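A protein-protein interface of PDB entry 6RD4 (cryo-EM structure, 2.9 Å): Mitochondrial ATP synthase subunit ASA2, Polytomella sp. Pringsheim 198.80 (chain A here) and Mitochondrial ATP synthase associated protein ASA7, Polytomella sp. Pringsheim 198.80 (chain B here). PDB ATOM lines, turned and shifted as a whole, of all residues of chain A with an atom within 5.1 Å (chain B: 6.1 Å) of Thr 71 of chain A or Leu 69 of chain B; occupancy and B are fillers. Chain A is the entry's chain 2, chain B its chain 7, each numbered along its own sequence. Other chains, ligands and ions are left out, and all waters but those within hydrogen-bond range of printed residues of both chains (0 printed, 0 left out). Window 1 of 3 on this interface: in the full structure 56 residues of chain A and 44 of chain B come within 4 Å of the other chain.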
ATOM      1  N   THR A  33     -10.878  16.516  -6.502  1.00  0.00           N
ATOM      2  CA  THR A  33     -10.678  17.829  -7.089  1.00  0.00           C
ATOM      3  C   THR A  33      -9.652  17.795  -8.203  1.00  0.00           C
ATOM      4  O   THR A  33      -9.883  18.375  -9.265  1.00  0.00           O
ATOM      5  CB  THR A  33     -10.244  18.825  -6.029  1.00  0.00           C
ATOM      6  OG1 THR A  33      -8.903  18.543  -5.635  1.00  0.00           O
ATOM      7  CG2 THR A  33     -11.113  18.681  -4.848  1.00  0.00           C
ATOM      8  N   GLN A  36     -11.402  16.608 -10.971  1.00  0.00           N
ATOM      9  CA  GLN A  36     -12.416  17.582 -11.393  1.00  0.00           C
ATOM     10  C   GLN A  36     -13.788  16.929 -11.606  1.00  0.00           C
ATOM     11  O   GLN A  36     -14.284  16.810 -12.723  1.00  0.00           O
ATOM     12  CB  GLN A  36     -11.952  18.324 -12.646  1.00  0.00           C
ATOM     13  CG  GLN A  36     -10.598  18.961 -12.501  1.00  0.00           C
ATOM     14  CD  GLN A  36     -10.156  19.625 -13.767  1.00  0.00           C
ATOM     15  OE1 GLN A  36     -10.943  20.285 -14.443  1.00  0.00           O
ATOM     16  NE2 GLN A  36      -8.898  19.435 -14.118  1.00  0.00           N
ATOM     17  N   VAL A  37     -14.398  16.529 -10.487  1.00  0.00           N
ATOM     18  CA  VAL A  37     -15.530  15.602 -10.470  1.00  0.00           C
ATOM     19  C   VAL A  37     -16.783  16.386 -10.071  1.00  0.00           C
ATOM     20  O   VAL A  37     -17.499  16.037  -9.127  1.00  0.00           O
ATOM     21  CB  VAL A  37     -15.245  14.388  -9.560  1.00  0.00           C
ATOM     22  CG1 VAL A  37     -16.258  13.257  -9.761  1.00  0.00           C
ATOM     23  CG2 VAL A  37     -13.912  13.836  -9.867  1.00  0.00           C
ATOM     24  N   LYS A  38     -16.987  17.545 -10.690  1.00  0.00           N
ATOM     25  CA  LYS A  38     -18.226  18.277 -10.456  1.00  0.00           C
ATOM     26  C   LYS A  38     -19.470  17.556 -10.957  1.00  0.00           C
ATOM     27  O   LYS A  38     -20.572  17.888 -10.516  1.00  0.00           O
ATOM     28  CB  LYS A  38     -18.172  19.643 -11.114  1.00  0.00           C
ATOM     29  CG  LYS A  38     -16.916  20.370 -10.835  1.00  0.00           C
ATOM     30  CD  LYS A  38     -16.811  20.722  -9.383  1.00  0.00           C
ATOM     31  CE  LYS A  38     -17.859  21.717  -9.006  1.00  0.00           C
ATOM     32  NZ  LYS A  38     -17.790  22.922  -9.845  1.00  0.00           N
ATOM     33  N   LEU A  66     -10.065  20.390   3.810  1.00  0.00           N
ATOM     34  CA  LEU A  66     -10.633  21.719   3.670  1.00  0.00           C
ATOM     35  C   LEU A  66     -10.137  22.410   2.416  1.00  0.00           C
ATOM     36  O   LEU A  66     -10.866  23.219   1.841  1.00  0.00           O
ATOM     37  CB  LEU A  66     -10.312  22.545   4.903  1.00  0.00           C
ATOM     38  CG  LEU A  66     -11.253  22.268   6.057  1.00  0.00           C
ATOM     39  CD1 LEU A  66     -10.846  23.050   7.249  1.00  0.00           C
ATOM     40  CD2 LEU A  66     -12.649  22.627   5.679  1.00  0.00           C
ATOM     41  N   TRP A  67      -8.920  22.096   1.972  1.00  0.00           N
ATOM     42  CA  TRP A  67      -8.471  22.545   0.660  1.00  0.00           C
ATOM     43  C   TRP A  67      -9.338  21.967  -0.436  1.00  0.00           C
ATOM     44  O   TRP A  67      -9.700  22.671  -1.375  1.00  0.00           O
ATOM     45  CB  TRP A  67      -7.017  22.144   0.422  1.00  0.00           C
ATOM     46  CG  TRP A  67      -6.503  22.518  -0.925  1.00  0.00           C
ATOM     47  CD1 TRP A  67      -5.923  23.684  -1.265  1.00  0.00           C
ATOM     48  CD2 TRP A  67      -6.522  21.721  -2.110  1.00  0.00           C
ATOM     49  NE1 TRP A  67      -5.585  23.678  -2.583  1.00  0.00           N
ATOM     50  CE2 TRP A  67      -5.950  22.480  -3.126  1.00  0.00           C
ATOM     51  CE3 TRP A  67      -6.975  20.437  -2.408  1.00  0.00           C
ATOM     52  CZ2 TRP A  67      -5.814  22.006  -4.413  1.00  0.00           C
ATOM     53  CZ3 TRP A  67      -6.845  19.976  -3.684  1.00  0.00           C
ATOM     54  CH2 TRP A  67      -6.272  20.753  -4.669  1.00  0.00           C
ATOM     55  N   ALA A  68      -9.693  20.694  -0.327  1.00  0.00           N
ATOM     56  CA  ALA A  68     -10.423  20.036  -1.400  1.00  0.00           C
ATOM     57  C   ALA A  68     -11.868  20.487  -1.447  1.00  0.00           C
ATOM     58  O   ALA A  68     -12.471  20.535  -2.519  1.00  0.00           O
ATOM     59  CB  ALA A  68     -10.341  18.534  -1.221  1.00  0.00           C
ATOM     60  N   ILE A  69     -12.443  20.803  -0.292  1.00  0.00           N
ATOM     61  CA  ILE A  69     -13.793  21.344  -0.243  1.00  0.00           C
ATOM     62  C   ILE A  69     -13.827  22.727  -0.871  1.00  0.00           C
ATOM     63  O   ILE A  69     -14.696  23.032  -1.691  1.00  0.00           O
ATOM     64  CB  ILE A  69     -14.279  21.370   1.214  1.00  0.00           C
ATOM     65  CG1 ILE A  69     -14.450  19.960   1.750  1.00  0.00           C
ATOM     66  CG2 ILE A  69     -15.564  22.106   1.337  1.00  0.00           C
ATOM     67  CD1 ILE A  69     -14.638  19.926   3.219  1.00  0.00           C
ATOM     68  N   ASN A  70     -12.843  23.558  -0.542  1.00  0.00           N
ATOM     69  CA  ASN A  70     -12.792  24.919  -1.045  1.00  0.00           C
ATOM     70  C   ASN A  70     -12.460  24.961  -2.525  1.00  0.00           C
ATOM     71  O   ASN A  70     -13.131  25.654  -3.291  1.00  0.00           O
ATOM     72  CB  ASN A  70     -11.760  25.703  -0.263  1.00  0.00           C
ATOM     73  CG  ASN A  70     -11.981  27.160  -0.352  1.00  0.00           C
ATOM     74  OD1 ASN A  70     -13.114  27.621  -0.344  1.00  0.00           O
ATOM     75  ND2 ASN A  70     -10.903  27.916  -0.446  1.00  0.00           N
ATOM     76  N   THR A  71     -11.428  24.232  -2.946  1.00  0.00           N
ATOM     77  CA  THR A  71     -11.011  24.247  -4.342  1.00  0.00           C
ATOM     78  C   THR A  71     -12.029  23.564  -5.233  1.00  0.00           C
ATOM     79  O   THR A  71     -12.279  24.013  -6.355  1.00  0.00           O
ATOM     80  CB  THR A  71      -9.661  23.571  -4.476  1.00  0.00           C
ATOM     81  OG1 THR A  71      -8.766  24.147  -3.529  1.00  0.00           O
ATOM     82  CG2 THR A  71      -9.101  23.743  -5.847  1.00  0.00           C
ATOM     83  N   GLY A  72     -12.644  22.496  -4.751  1.00  0.00           N
ATOM     84  CA  GLY A  72     -13.605  21.801  -5.567  1.00  0.00           C
ATOM     85  C   GLY A  72     -14.909  22.524  -5.738  1.00  0.00           C
ATOM     86  O   GLY A  72     -15.690  22.147  -6.612  1.00  0.00           O
ATOM     87  N   GLY A  73     -15.164  23.544  -4.934  1.00  0.00           N
ATOM     88  CA  GLY A  73     -16.397  24.286  -5.043  1.00  0.00           C
ATOM     89  C   GLY A  73     -17.585  23.577  -4.467  1.00  0.00           C
ATOM     90  O   GLY A  73     -18.711  23.862  -4.849  1.00  0.00           O
ATOM     91  N   THR B  19     -13.100  32.116  -5.387  1.00  0.00           N
ATOM     92  CA  THR B  19     -12.275  31.312  -4.505  1.00  0.00           C
ATOM     93  C   THR B  19     -10.836  31.384  -4.996  1.00  0.00           C
ATOM     94  O   THR B  19     -10.586  31.420  -6.202  1.00  0.00           O
ATOM     95  CB  THR B  19     -12.784  29.875  -4.481  1.00  0.00           C
ATOM     96  OG1 THR B  19     -14.183  29.881  -4.196  1.00  0.00           O
ATOM     97  CG2 THR B  19     -12.109  29.073  -3.404  1.00  0.00           C
ATOM     98  N   SER B  21      -7.990  29.301  -4.178  1.00  0.00           N
ATOM     99  CA  SER B  21      -7.146  28.161  -3.871  1.00  0.00           C
ATOM    100  C   SER B  21      -7.079  27.245  -5.079  1.00  0.00           C
ATOM    101  O   SER B  21      -7.985  27.206  -5.908  1.00  0.00           O
ATOM    102  CB  SER B  21      -7.655  27.389  -2.662  1.00  0.00           C
ATOM    103  OG  SER B  21      -8.768  26.606  -3.022  1.00  0.00           O
ATOM    104  N   GLY B  22      -5.978  26.503  -5.159  1.00  0.00           N
ATOM    105  CA  GLY B  22      -5.762  25.543  -6.221  1.00  0.00           C
ATOM    106  C   GLY B  22      -4.356  25.571  -6.777  1.00  0.00           C
ATOM    107  O   GLY B  22      -3.891  26.603  -7.264  1.00  0.00           O
ATOM    108  N   LEU B  23      -3.670  24.433  -6.688  1.00  0.00           N
ATOM    109  CA  LEU B  23      -2.309  24.173  -7.159  1.00  0.00           C
ATOM    110  C   LEU B  23      -1.252  25.091  -6.569  1.00  0.00           C
ATOM    111  O   LEU B  23      -0.131  25.122  -7.076  1.00  0.00           O
ATOM    112  CB  LEU B  23      -2.212  24.210  -8.683  1.00  0.00           C
ATOM    113  CG  LEU B  23      -2.652  22.956  -9.428  1.00  0.00           C
ATOM    114  CD1 LEU B  23      -2.058  22.955 -10.812  1.00  0.00           C
ATOM    115  CD2 LEU B  23      -2.260  21.691  -8.690  1.00  0.00           C
ATOM    116  N   ALA B  65      -6.937  25.528 -14.282  1.00  0.00           N
ATOM    117  CA  ALA B  65      -7.996  24.539 -14.413  1.00  0.00           C
ATOM    118  C   ALA B  65      -8.629  24.197 -13.082  1.00  0.00           C
ATOM    119  O   ALA B  65      -9.807  23.840 -13.042  1.00  0.00           O
ATOM    120  CB  ALA B  65      -7.469  23.260 -15.061  1.00  0.00           C
ATOM    121  N   LEU B  66      -7.869  24.298 -11.997  1.00  0.00           N
ATOM    122  CA  LEU B  66      -8.440  24.190 -10.668  1.00  0.00           C
ATOM    123  C   LEU B  66      -9.172  25.448 -10.240  1.00  0.00           C
ATOM    124  O   LEU B  66     -10.017  25.383  -9.342  1.00  0.00           O
ATOM    125  CB  LEU B  66      -7.355  23.879  -9.647  1.00  0.00           C
ATOM    126  CG  LEU B  66      -6.872  22.441  -9.549  1.00  0.00           C
ATOM    127  CD1 LEU B  66      -6.212  22.261  -8.216  1.00  0.00           C
ATOM    128  CD2 LEU B  66      -8.009  21.467  -9.715  1.00  0.00           C
ATOM    129  N   ARG B  67      -8.868  26.589 -10.845  1.00  0.00           N
ATOM    130  CA  ARG B  67      -9.564  27.804 -10.463  1.00  0.00           C
ATOM    131  C   ARG B  67     -10.939  27.881 -11.090  1.00  0.00           C
ATOM    132  O   ARG B  67     -11.826  28.534 -10.544  1.00  0.00           O
ATOM    133  CB  ARG B  67      -8.739  29.020 -10.845  1.00  0.00           C
ATOM    134  CG  ARG B  67      -7.385  29.039 -10.211  1.00  0.00           C
ATOM    135  CD  ARG B  67      -7.468  29.354  -8.748  1.00  0.00           C
ATOM    136  NE  ARG B  67      -8.292  30.527  -8.509  1.00  0.00           N
ATOM    137  CZ  ARG B  67      -7.871  31.780  -8.647  1.00  0.00           C
ATOM    138  NH1 ARG B  67      -6.631  32.037  -9.023  1.00  0.00           N
ATOM    139  NH2 ARG B  67      -8.701  32.783  -8.407  1.00  0.00           N
ATOM    140  N   LYS B  68     -11.147  27.219 -12.217  1.00  0.00           N
ATOM    141  CA  LYS B  68     -12.484  27.136 -12.776  1.00  0.00           C
ATOM    142  C   LYS B  68     -13.339  26.085 -12.100  1.00  0.00           C
ATOM    143  O   LYS B  68     -14.512  25.948 -12.459  1.00  0.00           O
ATOM    144  CB  LYS B  68     -12.432  26.823 -14.264  1.00  0.00           C
ATOM    145  CG  LYS B  68     -11.554  27.722 -15.068  1.00  0.00           C
ATOM    146  CD  LYS B  68     -11.788  27.470 -16.539  1.00  0.00           C
ATOM    147  CE  LYS B  68     -10.680  28.041 -17.381  1.00  0.00           C
ATOM    148  NZ  LYS B  68     -11.105  28.133 -18.793  1.00  0.00           N
ATOM    149  N   LEU B  69     -12.781  25.326 -11.159  1.00  0.00           N
ATOM    150  CA  LEU B  69     -13.545  24.261 -10.528  1.00  0.00           C
ATOM    151  C   LEU B  69     -14.578  24.820  -9.572  1.00  0.00           C
ATOM    152  O   LEU B  69     -15.725  24.368  -9.551  1.00  0.00           O
ATOM    153  CB  LEU B  69     -12.604  23.311  -9.807  1.00  0.00           C
ATOM    154  CG  LEU B  69     -13.072  21.870  -9.728  1.00  0.00           C
ATOM    155  CD1 LEU B  69     -13.405  21.376 -11.088  1.00  0.00           C
ATOM    156  CD2 LEU B  69     -11.979  21.060  -9.130  1.00  0.00           C
ATOM    157  N   SER B  70     -14.207  25.845  -8.815  1.00  0.00           N
ATOM    158  CA  SER B  70     -15.098  26.490  -7.868  1.00  0.00           C
ATOM    159  C   SER B  70     -15.929  27.583  -8.504  1.00  0.00           C
ATOM    160  O   SER B  70     -16.243  28.571  -7.840  1.00  0.00           O
ATOM    161  CB  SER B  70     -14.291  27.067  -6.715  1.00  0.00           C
ATOM    162  OG  SER B  70     -13.481  28.115  -7.185  1.00  0.00           O
ATOM    163  N   GLY B  71     -16.259  27.458  -9.780  1.00  0.00           N
ATOM    164  CA  GLY B  71     -17.051  28.458 -10.454  1.00  0.00           C
ATOM    165  C   GLY B  71     -18.522  28.159 -10.345  1.00  0.00           C
ATOM    166  O   GLY B  71     -19.317  29.033 -10.001  1.00  0.00           O
ATOM    167  N   SER B  72     -18.897  26.930 -10.666  1.00  0.00           N
ATOM    168  CA  SER B  72     -20.247  26.443 -10.443  1.00  0.00           C
ATOM    169  C   SER B  72     -20.211  25.502  -9.250  1.00  0.00           C
ATOM    170  O   SER B  72     -19.551  24.467  -9.300  1.00  0.00           O
ATOM    171  CB  SER B  72     -20.783  25.736 -11.681  1.00  0.00           C
ATOM    172  OG  SER B  72     -19.832  24.822 -12.178  1.00  0.00           O
ATOM    173  N   LYS B  73     -20.914  25.863  -8.188  1.00  0.00           N
ATOM    174  CA  LYS B  73     -20.790  25.152  -6.931  1.00  0.00           C
ATOM    175  C   LYS B  73     -21.598  23.864  -6.949  1.00  0.00           C
ATOM    176  O   LYS B  73     -22.553  23.719  -7.713  1.00  0.00           O
ATOM    177  CB  LYS B  73     -21.253  26.033  -5.782  1.00  0.00           C
ATOM    178  CG  LYS B  73     -20.584  27.379  -5.727  1.00  0.00           C
ATOM    179  CD  LYS B  73     -19.246  27.290  -5.075  1.00  0.00           C
ATOM    180  CE  LYS B  73     -18.429  28.525  -5.353  1.00  0.00           C
ATOM    181  NZ  LYS B  73     -19.275  29.726  -5.397  1.00  0.00           N
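Ala 68 of chain A touches none of the printed residues of chain B. Thr 71 of chain A touches just these residues of chain B: Ser 21 (2.5 Å), Gly 22 (3.8 Å), Leu 66 (3.97 Å), Leu 69 (3.5 Å) and Ser 70 (3.6 Å). Printed residues of chain A within 4 Å of Gly 22 of chain B: Trp 67 and Thr 71. Of the printed residues of chain A, Leu 69 of chain B touches Thr 33 (3.4 Å), Gln 36 (3.7 Å), Lys 38 (2.5 Å), Thr 71 (3.5 Å) and Gly 72 (3.7 Å). Of the printed residues of chain A, Ser 70 of chain B touches Asn 70, Thr 71 and Gly 73. The nearest residue of chain B that does not touch Thr 71 of chain A is Thr 19 of chain B (4.9 Å).
The backbone carbonyl oxygen (O) of Trp 67 of chain A is in hydrogen-bond range of the side-chain hydroxyl (OG1) of Thr 71 of chain A (2.8 Å). O of Thr 19 of chain B lies within hydrogen-bond range of NH2 of Arg 67 of chain B (3.2 Å).
Of the 12 printed residues of chain A, 8 touch a printed residue of chain B. Along chain A the printed residues that touch a printed residue of chain B span positions 33 to 73. Hydrophobic or aromatic side chains of chain B within 4 Å of the printed part of chain A: Leu 66 and Leu 69. Among the printed residues, no Asp or Glu carboxylate lies within 4 Å of a Lys or Arg side-chain nitrogen of the other chain.
The side-chain amino group of Lys 38 of chain A is in hydrogen-bond range of the backbone carbonyl oxygen of Leu 69 of chain B (2.5 Å). The backbone carbonyl oxygen of Ser 72 of chain B lies within hydrogen-bond range of the side-chain amino group of Lys 38 of chain A (2.4 Å). The side-chain hydroxyl (OG) of Ser 21 of chain B sits at hydrogen-bond distance from the side-chain hydroxyl (OG1) of Thr 71 of chain A.
O of Ala 65 of chain B touches OE1 of Gln 36 of chain A (3.99 Å). Leu 69 of chain B touches Gln 36 of chain A. NE1 of Trp 67 of chain A touches N of Gly 22 of chain B, at 3.8 Å. Asn 70 of chain A touches Thr 19 of chain B. Gly 22 of chain B touches Thr 71 of chain A (CA to CG2, 3.8 Å). Leu 66 of chain B touches Thr 71 of chain A (O to CG2, 3.97 Å). Ser 70 of chain B touches Thr 71 of chain A (N to O, 3.6 Å). O of Gly 72 of chain A touches O of Leu 69 of chain B, at 3.7 Å. Ser 70 of chain B touches Gly 73 of chain A (CA to CA, 3.8 Å). Lys 73 of chain B touches Gly 73 of chain A (CA to O, 3.2 Å).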
